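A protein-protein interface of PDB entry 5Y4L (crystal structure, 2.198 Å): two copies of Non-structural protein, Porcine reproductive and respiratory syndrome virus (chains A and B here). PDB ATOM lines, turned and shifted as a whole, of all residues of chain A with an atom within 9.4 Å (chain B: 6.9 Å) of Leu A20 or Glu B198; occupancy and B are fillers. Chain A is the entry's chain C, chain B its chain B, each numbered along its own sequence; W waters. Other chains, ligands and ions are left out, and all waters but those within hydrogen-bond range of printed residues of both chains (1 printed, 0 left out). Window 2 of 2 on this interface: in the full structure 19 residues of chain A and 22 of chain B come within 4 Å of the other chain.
The backbone carbonyl oxygen (O) of Val B181 is in hydrogen-bond range of the backbone NH (N) of Val B199. The side-chain hydroxyl (OG1) of Thr B196 lies within hydrogen-bond range of the backbone carbonyl oxygen (O) of Glu B198 (2.9 Å). The backbone carbonyl oxygen (O) of Lys A17 is in hydrogen-bond range of the side-chain hydroxyl (OG1) of Thr A15. The side-chain hydroxyl of Thr A15 is in hydrogen-bond range of the backbone NH of Val A109 (2.9 Å). The side-chain amide oxygen (OD1) of Asn A21 is in hydrogen-bond range of the side-chain hydroxyl (OG) of Ser A19 (2.9 Å). The side-chain hydroxyl (OG) of Ser A19 lies within hydrogen-bond range of the side-chain hydroxyl (OG1) of Thr A22 (2.8 Å).
Among the printed residues, merely in contact across the chains: Pro A18 with Pro B182 (3.2 Å), Ser A19 with Lys B180 (3.5 Å), Leu A20 with Glu B198 (3.7 Å), Val A109 with Val B181 (3.7 Å), Leu A20 with Pro B182 (3.8 Å), Thr A15 with Val B181 (3.96 Å) and Lys A17 with Val B181 (3.99 Å).
Of the printed residues of chain B, Lys A17 touches Val B181. Printed residues of chain B within 4 Å of Pro A18: Pro B182 (3.2 Å). Phe A36 touches none of the printed residues of chain B. No residue of chain A comes within 4 Å of Cys B197. Glu B198 touches one residue of chain A. No residue of chain A comes within 4 Å of Val B199. The nearest residue of chain B that does not touch Leu A20 is Lys B180 (4.4 Å). The nearest printed residue of chain A that does not touch Val B181 is Ser A19 (4.1 Å).
Printed residues of chain A that touch a printed residue of chain B: Thr A15, Lys A17, Pro A18, Ser A19, Leu A20 and Val A109. Hydrophobic or aromatic side chains of chain A that line the printed part of chain B: Leu A20 and Val A109. Along chain A the printed residues that touch a printed residue of chain B span positions 15 to 109. Among the printed residues, 7 pairs touch across the chains. Among the printed residues, no Asp or Glu carboxylate lies within 4 Å of a Lys or Arg side-chain nitrogen of the other chain.
No position is printed for both chains. Of the 7 pairs that touch across the chains among the printed residues, none has its exchanged pair printed and touching as well.
Water W1 bridges the backbone NH of Lys A17 (2.8 Å) and the backbone carbonyl oxygen of Pro B182 (2.9 Å).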
ATOM      1  N   THR A  15      20.269   7.806 -25.663  1.00  0.00           N
ATOM      2  CA  THR A  15      20.308   9.271 -25.696  1.00  0.00           C
ATOM      3  C   THR A  15      21.332   9.769 -24.675  1.00  0.00           C
ATOM      4  O   THR A  15      21.738   9.026 -23.782  1.00  0.00           O
ATOM      5  CB  THR A  15      18.915   9.918 -25.429  1.00  0.00           C
ATOM      6  OG1 THR A  15      18.407   9.516 -24.154  1.00  0.00           O
ATOM      7  CG2 THR A  15      17.921   9.517 -26.514  1.00  0.00           C
ATOM      8  N   LYS A  17      20.925  12.419 -22.668  1.00  0.00           N
ATOM      9  CA  LYS A  17      20.181  12.754 -21.459  1.00  0.00           C
ATOM     10  C   LYS A  17      18.878  11.956 -21.339  1.00  0.00           C
ATOM     11  O   LYS A  17      18.249  11.617 -22.345  1.00  0.00           O
ATOM     12  CB  LYS A  17      19.885  14.261 -21.418  1.00  0.00           C
ATOM     13  CG  LYS A  17      21.143  15.115 -21.303  1.00  0.00           C
ATOM     14  CD  LYS A  17      20.824  16.533 -20.867  1.00  0.00           C
ATOM     15  CE  LYS A  17      22.095  17.365 -20.729  1.00  0.00           C
ATOM     16  NZ  LYS A  17      23.143  16.694 -19.893  1.00  0.00           N
ATOM     17  N   PRO A  18      18.479  11.646 -20.095  1.00  0.00           N
ATOM     18  CA  PRO A  18      17.208  10.986 -19.771  1.00  0.00           C
ATOM     19  C   PRO A  18      16.008  11.788 -20.227  1.00  0.00           C
ATOM     20  O   PRO A  18      16.132  12.972 -20.520  1.00  0.00           O
ATOM     21  CB  PRO A  18      17.237  10.889 -18.235  1.00  0.00           C
ATOM     22  CG  PRO A  18      18.304  11.841 -17.791  1.00  0.00           C
ATOM     23  CD  PRO A  18      19.314  11.851 -18.899  1.00  0.00           C
ATOM     24  N   SER A  19      14.847  11.154 -20.289  1.00  0.00           N
ATOM     25  CA  SER A  19      13.623  11.915 -20.484  1.00  0.00           C
ATOM     26  C   SER A  19      13.292  12.742 -19.219  1.00  0.00           C
ATOM     27  O   SER A  19      13.841  12.512 -18.132  1.00  0.00           O
ATOM     28  CB  SER A  19      12.461  10.996 -20.845  1.00  0.00           C
ATOM     29  OG  SER A  19      12.045  10.225 -19.734  1.00  0.00           O
ATOM     30  N   LEU A  20      12.393  13.708 -19.379  1.00  0.00           N
ATOM     31  CA  LEU A  20      12.031  14.620 -18.294  1.00  0.00           C
ATOM     32  C   LEU A  20      11.334  13.924 -17.117  1.00  0.00           C
ATOM     33  O   LEU A  20      11.501  14.340 -15.961  1.00  0.00           O
ATOM     34  CB  LEU A  20      11.133  15.748 -18.832  1.00  0.00           C
ATOM     35  CG  LEU A  20      11.771  16.706 -19.849  1.00  0.00           C
ATOM     36  CD1 LEU A  20      10.756  17.738 -20.321  1.00  0.00           C
ATOM     37  CD2 LEU A  20      13.014  17.386 -19.279  1.00  0.00           C
ATOM     38  N   ASN A  21      10.561  12.874 -17.399  1.00  0.00           N
ATOM     39  CA  ASN A  21       9.863  12.150 -16.332  1.00  0.00           C
ATOM     40  C   ASN A  21      10.703  11.013 -15.744  1.00  0.00           C
ATOM     41  O   ASN A  21      10.227  10.252 -14.909  1.00  0.00           O
ATOM     42  CB  ASN A  21       8.524  11.603 -16.837  1.00  0.00           C
ATOM     43  CG  ASN A  21       8.688  10.654 -18.012  1.00  0.00           C
ATOM     44  OD1 ASN A  21       9.327  10.986 -19.003  1.00  0.00           O
ATOM     45  ND2 ASN A  21       8.127   9.466 -17.896  1.00  0.00           N
ATOM     46  N   THR A  22      11.956  10.896 -16.174  1.00  0.00           N
ATOM     47  CA  THR A  22      12.825   9.863 -15.620  1.00  0.00           C
ATOM     48  C   THR A  22      13.393  10.390 -14.328  1.00  0.00           C
ATOM     49  O   THR A  22      13.668  11.582 -14.215  1.00  0.00           O
ATOM     50  CB  THR A  22      13.976   9.470 -16.587  1.00  0.00           C
ATOM     51  OG1 THR A  22      13.432   8.816 -17.737  1.00  0.00           O
ATOM     52  CG2 THR A  22      14.957   8.530 -15.917  1.00  0.00           C
ATOM     53  N   VAL A  23      13.573   9.510 -13.349  1.00  0.00           N
ATOM     54  CA  VAL A  23      14.114   9.917 -12.059  1.00  0.00           C
ATOM     55  C   VAL A  23      15.228   8.978 -11.604  1.00  0.00           C
ATOM     56  O   VAL A  23      15.324   7.839 -12.064  1.00  0.00           O
ATOM     57  CB  VAL A  23      13.002   9.971 -10.984  1.00  0.00           C
ATOM     58  CG1 VAL A  23      12.049  11.134 -11.264  1.00  0.00           C
ATOM     59  CG2 VAL A  23      12.239   8.642 -10.939  1.00  0.00           C
ATOM     60  N   ASN A  24      16.092   9.481 -10.731  1.00  0.00           N
ATOM     61  CA  ASN A  24      17.009   8.633  -9.988  1.00  0.00           C
ATOM     62  C   ASN A  24      16.291   8.064  -8.775  1.00  0.00           C
ATOM     63  O   ASN A  24      15.397   8.704  -8.215  1.00  0.00           O
ATOM     64  CB  ASN A  24      18.247   9.403  -9.549  1.00  0.00           C
ATOM     65  CG  ASN A  24      19.286   9.488 -10.634  1.00  0.00           C
ATOM     66  OD1 ASN A  24      20.190   8.657 -10.706  1.00  0.00           O
ATOM     67  ND2 ASN A  24      19.161  10.491 -11.494  1.00  0.00           N
ATOM     68  N   GLY A  33      13.855   5.129 -12.368  1.00  0.00           N
ATOM     69  CA  GLY A  33      12.419   5.037 -12.256  1.00  0.00           C
ATOM     70  C   GLY A  33      11.851   6.109 -13.146  1.00  0.00           C
ATOM     71  O   GLY A  33      12.598   6.868 -13.762  1.00  0.00           O
ATOM     72  N   GLY A  34      10.533   6.178 -13.220  1.00  0.00           N
ATOM     73  CA  GLY A  34       9.880   7.217 -13.985  1.00  0.00           C
ATOM     74  C   GLY A  34       8.532   7.605 -13.409  1.00  0.00           C
ATOM     75  O   GLY A  34       7.963   6.906 -12.558  1.00  0.00           O
ATOM     76  N   VAL A  35       8.011   8.721 -13.902  1.00  0.00           N
ATOM     77  CA  VAL A  35       6.781   9.299 -13.382  1.00  0.00           C
ATOM     78  C   VAL A  35       5.759   9.373 -14.498  1.00  0.00           C
ATOM     79  O   VAL A  35       6.074   9.842 -15.597  1.00  0.00           O
ATOM     80  CB  VAL A  35       7.035  10.709 -12.791  1.00  0.00           C
ATOM     81  CG1 VAL A  35       5.737  11.347 -12.337  1.00  0.00           C
ATOM     82  CG2 VAL A  35       8.038  10.634 -11.653  1.00  0.00           C
ATOM     83  N   PHE A  36       4.548   8.891 -14.231  1.00  0.00           N
ATOM     84  CA  PHE A  36       3.495   8.871 -15.240  1.00  0.00           C
ATOM     85  C   PHE A  36       2.133   9.215 -14.642  1.00  0.00           C
ATOM     86  O   PHE A  36       1.919   9.104 -13.433  1.00  0.00           O
ATOM     87  CB  PHE A  36       3.402   7.499 -15.912  1.00  0.00           C
ATOM     88  CG  PHE A  36       4.697   7.019 -16.537  1.00  0.00           C
ATOM     89  CD1 PHE A  36       5.683   6.425 -15.763  1.00  0.00           C
ATOM     90  CD2 PHE A  36       4.899   7.119 -17.906  1.00  0.00           C
ATOM     91  CE1 PHE A  36       6.861   5.973 -16.336  1.00  0.00           C
ATOM     92  CE2 PHE A  36       6.069   6.666 -18.481  1.00  0.00           C
ATOM     93  CZ  PHE A  36       7.054   6.095 -17.691  1.00  0.00           C
ATOM     94  N   SER A  59      14.893  11.310  -6.914  1.00  0.00           N
ATOM     95  CA  SER A  59      15.352  12.635  -7.324  1.00  0.00           C
ATOM     96  C   SER A  59      15.276  12.853  -8.834  1.00  0.00           C
ATOM     97  O   SER A  59      15.373  11.919  -9.627  1.00  0.00           O
ATOM     98  CB  SER A  59      16.783  12.871  -6.850  1.00  0.00           C
ATOM     99  OG  SER A  59      17.650  11.891  -7.383  1.00  0.00           O
ATOM    100  N   GLY A  60      15.114  14.109  -9.219  1.00  0.00           N
ATOM    101  CA  GLY A  60      15.085  14.488 -10.615  1.00  0.00           C
ATOM    102  C   GLY A  60      15.168  15.992 -10.689  1.00  0.00           C
ATOM    103  O   GLY A  60      15.272  16.660  -9.665  1.00  0.00           O
ATOM    104  N   VAL A  61      15.126  16.533 -11.898  1.00  0.00           N
ATOM    105  CA  VAL A  61      15.225  17.975 -12.059  1.00  0.00           C
ATOM    106  C   VAL A  61      14.013  18.654 -11.415  1.00  0.00           C
ATOM    107  O   VAL A  61      12.876  18.437 -11.821  1.00  0.00           O
ATOM    108  CB  VAL A  61      15.351  18.371 -13.546  1.00  0.00           C
ATOM    109  CG1 VAL A  61      15.302  19.879 -13.694  1.00  0.00           C
ATOM    110  CG2 VAL A  61      16.657  17.805 -14.142  1.00  0.00           C
ATOM    111  N   GLY A  62      14.277  19.458 -10.384  1.00  0.00           N
ATOM    112  CA  GLY A  62      13.225  20.121  -9.633  1.00  0.00           C
ATOM    113  C   GLY A  62      12.442  19.170  -8.743  1.00  0.00           C
ATOM    114  O   GLY A  62      11.310  19.465  -8.359  1.00  0.00           O
ATOM    115  N   PHE A  63      13.044  18.030  -8.411  1.00  0.00           N
ATOM    116  CA  PHE A  63      12.400  17.048  -7.539  1.00  0.00           C
ATOM    117  C   PHE A  63      13.385  16.252  -6.685  1.00  0.00           C
ATOM    118  O   PHE A  63      14.501  15.955  -7.109  1.00  0.00           O
ATOM    119  CB  PHE A  63      11.560  16.079  -8.363  1.00  0.00           C
ATOM    120  CG  PHE A  63      10.563  15.311  -7.551  1.00  0.00           C
ATOM    121  CD1 PHE A  63      10.915  14.119  -6.938  1.00  0.00           C
ATOM    122  CD2 PHE A  63       9.266  15.782  -7.400  1.00  0.00           C
ATOM    123  CE1 PHE A  63       9.990  13.408  -6.182  1.00  0.00           C
ATOM    124  CE2 PHE A  63       8.336  15.079  -6.652  1.00  0.00           C
ATOM    125  CZ  PHE A  63       8.698  13.889  -6.043  1.00  0.00           C
ATOM    126  N   TRP A  83       4.841  16.074  -7.784  1.00  0.00           N
ATOM    127  CA  TRP A  83       5.485  16.227  -9.091  1.00  0.00           C
ATOM    128  C   TRP A  83       4.854  17.372  -9.898  1.00  0.00           C
ATOM    129  O   TRP A  83       3.686  17.290 -10.291  1.00  0.00           O
ATOM    130  CB  TRP A  83       5.391  14.904  -9.869  1.00  0.00           C
ATOM    131  CG  TRP A  83       6.204  14.846 -11.120  1.00  0.00           C
ATOM    132  CD1 TRP A  83       5.771  15.058 -12.399  1.00  0.00           C
ATOM    133  CD2 TRP A  83       7.602  14.550 -11.214  1.00  0.00           C
ATOM    134  NE1 TRP A  83       6.816  14.902 -13.285  1.00  0.00           N
ATOM    135  CE2 TRP A  83       7.951  14.597 -12.581  1.00  0.00           C
ATOM    136  CE3 TRP A  83       8.590  14.247 -10.275  1.00  0.00           C
ATOM    137  CZ2 TRP A  83       9.245  14.362 -13.026  1.00  0.00           C
ATOM    138  CZ3 TRP A  83       9.871  14.012 -10.719  1.00  0.00           C
ATOM    139  CH2 TRP A  83      10.190  14.075 -12.083  1.00  0.00           C
ATOM    140  N   GLN A  84       5.610  18.442 -10.136  1.00  0.00           N
ATOM    141  CA  GLN A  84       5.055  19.561 -10.900  1.00  0.00           C
ATOM    142  C   GLN A  84       5.416  19.444 -12.380  1.00  0.00           C
ATOM    143  O   GLN A  84       4.811  20.100 -13.233  1.00  0.00           O
ATOM    144  CB  GLN A  84       5.525  20.911 -10.340  1.00  0.00           C
ATOM    145  CG  GLN A  84       4.740  22.108 -10.906  1.00  0.00           C
ATOM    146  CD  GLN A  84       4.763  23.335 -10.007  1.00  0.00           C
ATOM    147  OE1 GLN A  84       4.241  23.310  -8.891  1.00  0.00           O
ATOM    148  NE2 GLN A  84       5.366  24.419 -10.496  1.00  0.00           N
ATOM    149  N   GLY A  85       6.384  18.583 -12.684  1.00  0.00           N
ATOM    150  CA  GLY A  85       6.790  18.352 -14.060  1.00  0.00           C
ATOM    151  C   GLY A  85       5.778  17.595 -14.908  1.00  0.00           C
ATOM    152  O   GLY A  85       4.664  17.290 -14.479  1.00  0.00           O
ATOM    153  N   VAL A  86       6.182  17.286 -16.130  1.00  0.00           N
ATOM    154  CA  VAL A  86       5.360  16.514 -17.051  1.00  0.00           C
ATOM    155  C   VAL A  86       5.174  15.076 -16.541  1.00  0.00           C
ATOM    156  O   VAL A  86       6.120  14.431 -16.084  1.00  0.00           O
ATOM    157  CB  VAL A  86       5.984  16.504 -18.476  1.00  0.00           C
ATOM    158  CG1 VAL A  86       7.428  15.978 -18.440  1.00  0.00           C
ATOM    159  CG2 VAL A  86       5.132  15.701 -19.440  1.00  0.00           C
ATOM    160  N   ALA A  87       3.943  14.586 -16.591  1.00  0.00           N
ATOM    161  CA  ALA A  87       3.671  13.202 -16.231  1.00  0.00           C
ATOM    162  C   ALA A  87       2.857  12.564 -17.342  1.00  0.00           C
ATOM    163  O   ALA A  87       1.627  12.603 -17.315  1.00  0.00           O
ATOM    164  CB  ALA A  87       2.943  13.123 -14.907  1.00  0.00           C
ATOM    165  N   PRO A  88       3.545  11.977 -18.337  1.00  0.00           N
ATOM    166  CA  PRO A  88       2.857  11.460 -19.525  1.00  0.00           C
ATOM    167  C   PRO A  88       1.781  10.456 -19.154  1.00  0.00           C
ATOM    168  O   PRO A  88       1.959   9.699 -18.202  1.00  0.00           O
ATOM    169  CB  PRO A  88       3.982  10.796 -20.331  1.00  0.00           C
ATOM    170  CG  PRO A  88       5.232  11.453 -19.857  1.00  0.00           C
ATOM    171  CD  PRO A  88       4.998  11.753 -18.397  1.00  0.00           C
ATOM    172  N   LEU A 104      13.546   3.761 -20.139  1.00  0.00           N
ATOM    173  CA  LEU A 104      13.808   5.126 -19.675  1.00  0.00           C
ATOM    174  C   LEU A 104      14.780   5.103 -18.510  1.00  0.00           C
ATOM    175  O   LEU A 104      14.355   5.198 -17.361  1.00  0.00           O
ATOM    176  CB  LEU A 104      12.503   5.828 -19.262  1.00  0.00           C
ATOM    177  CG  LEU A 104      11.630   6.334 -20.423  1.00  0.00           C
ATOM    178  CD1 LEU A 104      11.276   5.231 -21.425  1.00  0.00           C
ATOM    179  CD2 LEU A 104      10.361   7.024 -19.929  1.00  0.00           C
ATOM    180  N   THR A 105      16.078   4.966 -18.792  1.00  0.00           N
ATOM    181  CA  THR A 105      17.077   4.872 -17.715  1.00  0.00           C
ATOM    182  C   THR A 105      17.540   6.255 -17.266  1.00  0.00           C
ATOM    183  O   THR A 105      17.302   7.253 -17.959  1.00  0.00           O
ATOM    184  CB  THR A 105      18.316   4.058 -18.134  1.00  0.00           C
ATOM    185  OG1 THR A 105      19.277   4.916 -18.773  1.00  0.00           O
ATOM    186  CG2 THR A 105      17.923   2.943 -19.079  1.00  0.00           C
ATOM    187  N   GLY A 108      19.800   7.905 -19.764  1.00  0.00           N
ATOM    188  CA  GLY A 108      19.270   8.081 -21.107  1.00  0.00           C
ATOM    189  C   GLY A 108      18.339   6.979 -21.574  1.00  0.00           C
ATOM    190  O   GLY A 108      18.326   5.885 -21.009  1.00  0.00           O
ATOM    191  N   VAL A 109      17.555   7.274 -22.606  1.00  0.00           N
ATOM    192  CA  VAL A 109      16.651   6.293 -23.183  1.00  0.00           C
ATOM    193  C   VAL A 109      17.345   5.322 -24.153  1.00  0.00           C
ATOM    194  O   VAL A 109      17.935   5.737 -25.150  1.00  0.00           O
ATOM    195  CB  VAL A 109      15.507   6.971 -23.919  1.00  0.00           C
ATOM    196  CG1 VAL A 109      14.523   5.915 -24.481  1.00  0.00           C
ATOM    197  CG2 VAL A 109      14.802   7.951 -22.987  1.00  0.00           C
ATOM    198  N   LEU B 169      12.454  21.257 -36.930  1.00  0.00           N
ATOM    199  CA  LEU B 169      12.832  20.107 -36.117  1.00  0.00           C
ATOM    200  C   LEU B 169      11.605  19.336 -35.628  1.00  0.00           C
ATOM    201  O   LEU B 169      11.625  18.106 -35.528  1.00  0.00           O
ATOM    202  CB  LEU B 169      13.676  20.551 -34.925  1.00  0.00           C
ATOM    203  CG  LEU B 169      14.168  19.434 -34.008  1.00  0.00           C
ATOM    204  CD1 LEU B 169      15.040  18.434 -34.774  1.00  0.00           C
ATOM    205  CD2 LEU B 169      14.929  19.999 -32.857  1.00  0.00           C
ATOM    206  N   SER B 170      10.533  20.067 -35.343  1.00  0.00           N
ATOM    207  CA  SER B 170       9.306  19.452 -34.891  1.00  0.00           C
ATOM    208  C   SER B 170       8.684  18.574 -35.968  1.00  0.00           C
ATOM    209  O   SER B 170       8.087  17.535 -35.681  1.00  0.00           O
ATOM    210  CB  SER B 170       8.300  20.530 -34.461  1.00  0.00           C
ATOM    211  OG  SER B 170       7.892  21.303 -35.578  1.00  0.00           O
ATOM    212  N   SER B 173      10.546  15.368 -36.243  1.00  0.00           N
ATOM    213  CA  SER B 173      10.261  14.544 -35.068  1.00  0.00           C
ATOM    214  C   SER B 173       9.119  13.549 -35.267  1.00  0.00           C
ATOM    215  O   SER B 173       9.089  12.471 -34.660  1.00  0.00           O
ATOM    216  CB  SER B 173       9.930  15.444 -33.877  1.00  0.00           C
ATOM    217  OG  SER B 173      11.055  16.204 -33.471  1.00  0.00           O
ATOM    218  N   LYS B 180       9.870  11.894 -25.441  1.00  0.00           N
ATOM    219  CA  LYS B 180      10.579  13.111 -25.769  1.00  0.00           C
ATOM    220  C   LYS B 180      11.728  13.254 -24.787  1.00  0.00           C
ATOM    221  O   LYS B 180      11.608  12.891 -23.619  1.00  0.00           O
ATOM    222  CB  LYS B 180       9.633  14.311 -25.761  1.00  0.00           C
ATOM    223  CG  LYS B 180       9.170  14.700 -27.181  1.00  0.00           C
ATOM    224  CD  LYS B 180       7.757  15.282 -27.208  1.00  0.00           C
ATOM    225  CE  LYS B 180       6.696  14.190 -27.052  1.00  0.00           C
ATOM    226  NZ  LYS B 180       5.296  14.723 -27.018  1.00  0.00           N
ATOM    227  N   VAL B 181      12.881  13.687 -25.278  1.00  0.00           N
ATOM    228  CA  VAL B 181      14.030  13.898 -24.411  1.00  0.00           C
ATOM    229  C   VAL B 181      14.712  15.202 -24.827  1.00  0.00           C
ATOM    230  O   VAL B 181      14.585  15.646 -25.976  1.00  0.00           O
ATOM    231  CB  VAL B 181      15.056  12.726 -24.456  1.00  0.00           C
ATOM    232  CG1 VAL B 181      14.362  11.364 -24.462  1.00  0.00           C
ATOM    233  CG2 VAL B 181      16.022  12.881 -25.654  1.00  0.00           C
ATOM    234  N   PRO B 182      15.430  15.834 -23.892  1.00  0.00           N
ATOM    235  CA  PRO B 182      16.106  17.085 -24.247  1.00  0.00           C
ATOM    236  C   PRO B 182      17.287  16.867 -25.186  1.00  0.00           C
ATOM    237  O   PRO B 182      18.041  15.891 -25.036  1.00  0.00           O
ATOM    238  CB  PRO B 182      16.592  17.620 -22.895  1.00  0.00           C
ATOM    239  CG  PRO B 182      15.813  16.841 -21.856  1.00  0.00           C
ATOM    240  CD  PRO B 182      15.591  15.507 -22.468  1.00  0.00           C
ATOM    241  N   LEU B 183      17.430  17.772 -26.151  1.00  0.00           N
ATOM    242  CA  LEU B 183      18.642  17.856 -26.960  1.00  0.00           C
ATOM    243  C   LEU B 183      19.787  18.258 -26.052  1.00  0.00           C
ATOM    244  O   LEU B 183      19.690  19.245 -25.319  1.00  0.00           O
ATOM    245  CB  LEU B 183      18.481  18.869 -28.090  1.00  0.00           C
ATOM    246  CG  LEU B 183      17.401  18.627 -29.136  1.00  0.00           C
ATOM    247  CD1 LEU B 183      16.925  19.952 -29.677  1.00  0.00           C
ATOM    248  CD2 LEU B 183      17.927  17.761 -30.263  1.00  0.00           C
ATOM    249  N   ASP B 195      12.847  24.597 -33.673  1.00  0.00           N
ATOM    250  CA  ASP B 195      11.626  25.098 -33.057  1.00  0.00           C
ATOM    251  C   ASP B 195      11.210  24.298 -31.800  1.00  0.00           C
ATOM    252  O   ASP B 195      10.076  24.403 -31.333  1.00  0.00           O
ATOM    253  CB  ASP B 195      10.491  25.111 -34.089  1.00  0.00           C
ATOM    254  CG  ASP B 195      10.064  23.717 -34.520  1.00  0.00           C
ATOM    255  OD1 ASP B 195      10.832  22.747 -34.314  1.00  0.00           O
ATOM    256  OD2 ASP B 195       8.954  23.596 -35.082  1.00  0.00           O
ATOM    257  N   THR B 196      12.138  23.513 -31.255  1.00  0.00           N
ATOM    258  CA  THR B 196      11.924  22.791 -29.994  1.00  0.00           C
ATOM    259  C   THR B 196      13.276  22.419 -29.435  1.00  0.00           C
ATOM    260  O   THR B 196      14.255  22.344 -30.181  1.00  0.00           O
ATOM    261  CB  THR B 196      11.079  21.509 -30.169  1.00  0.00           C
ATOM    262  OG1 THR B 196      11.053  20.781 -28.935  1.00  0.00           O
ATOM    263  CG2 THR B 196      11.692  20.614 -31.244  1.00  0.00           C
ATOM    264  N   CYS B 197      13.351  22.190 -28.130  1.00  0.00           N
ATOM    265  CA  CYS B 197      14.619  21.773 -27.538  1.00  0.00           C
ATOM    266  C   CYS B 197      14.445  20.362 -26.982  1.00  0.00           C
ATOM    267  O   CYS B 197      15.314  19.830 -26.301  1.00  0.00           O
ATOM    268  CB  CYS B 197      15.064  22.742 -26.441  1.00  0.00           C
ATOM    269  SG  CYS B 197      15.488  24.396 -27.032  1.00  0.00           S
ATOM    270  N   GLU B 198      13.315  19.746 -27.297  1.00  0.00           N
ATOM    271  CA  GLU B 198      13.128  18.333 -26.975  1.00  0.00           C
ATOM    272  C   GLU B 198      12.671  17.552 -28.195  1.00  0.00           C
ATOM    273  O   GLU B 198      11.954  18.069 -29.054  1.00  0.00           O
ATOM    274  CB  GLU B 198      12.133  18.155 -25.826  1.00  0.00           C
ATOM    275  CG  GLU B 198      10.752  18.700 -26.097  1.00  0.00           C
ATOM    276  CD  GLU B 198       9.825  18.528 -24.903  1.00  0.00           C
ATOM    277  OE1 GLU B 198      10.231  18.938 -23.797  1.00  0.00           O
ATOM    278  OE2 GLU B 198       8.687  18.025 -25.077  1.00  0.00           O
ATOM    279  N   VAL B 199      13.071  16.290 -28.241  1.00  0.00           N
ATOM    280  CA  VAL B 199      12.921  15.473 -29.434  1.00  0.00           C
ATOM    281  C   VAL B 199      12.741  13.999 -29.034  1.00  0.00           C
ATOM    282  O   VAL B 199      13.336  13.562 -28.047  1.00  0.00           O
ATOM    283  CB  VAL B 199      14.156  15.690 -30.346  1.00  0.00           C
ATOM    284  CG1 VAL B 199      14.846  14.393 -30.689  1.00  0.00           C
ATOM    285  CG2 VAL B 199      13.767  16.473 -31.592  1.00  0.00           C
ATOM    286  N   PRO B 200      11.900  13.236 -29.769  1.00  0.00           N
ATOM    287  CA  PRO B 200      11.743  11.804 -29.458  1.00  0.00           C
ATOM    288  C   PRO B 200      13.101  11.108 -29.396  1.00  0.00           C
ATOM    289  O   PRO B 200      13.998  11.481 -30.157  1.00  0.00           O
ATOM    290  CB  PRO B 200      10.904  11.269 -30.628  1.00  0.00           C
ATOM    291  CG  PRO B 200      10.194  12.479 -31.155  1.00  0.00           C
ATOM    292  CD  PRO B 200      11.152  13.623 -30.975  1.00  0.00           C
HETATM  293  O   HOH W   1      19.581  13.408 -24.968  1.00  0.00           O
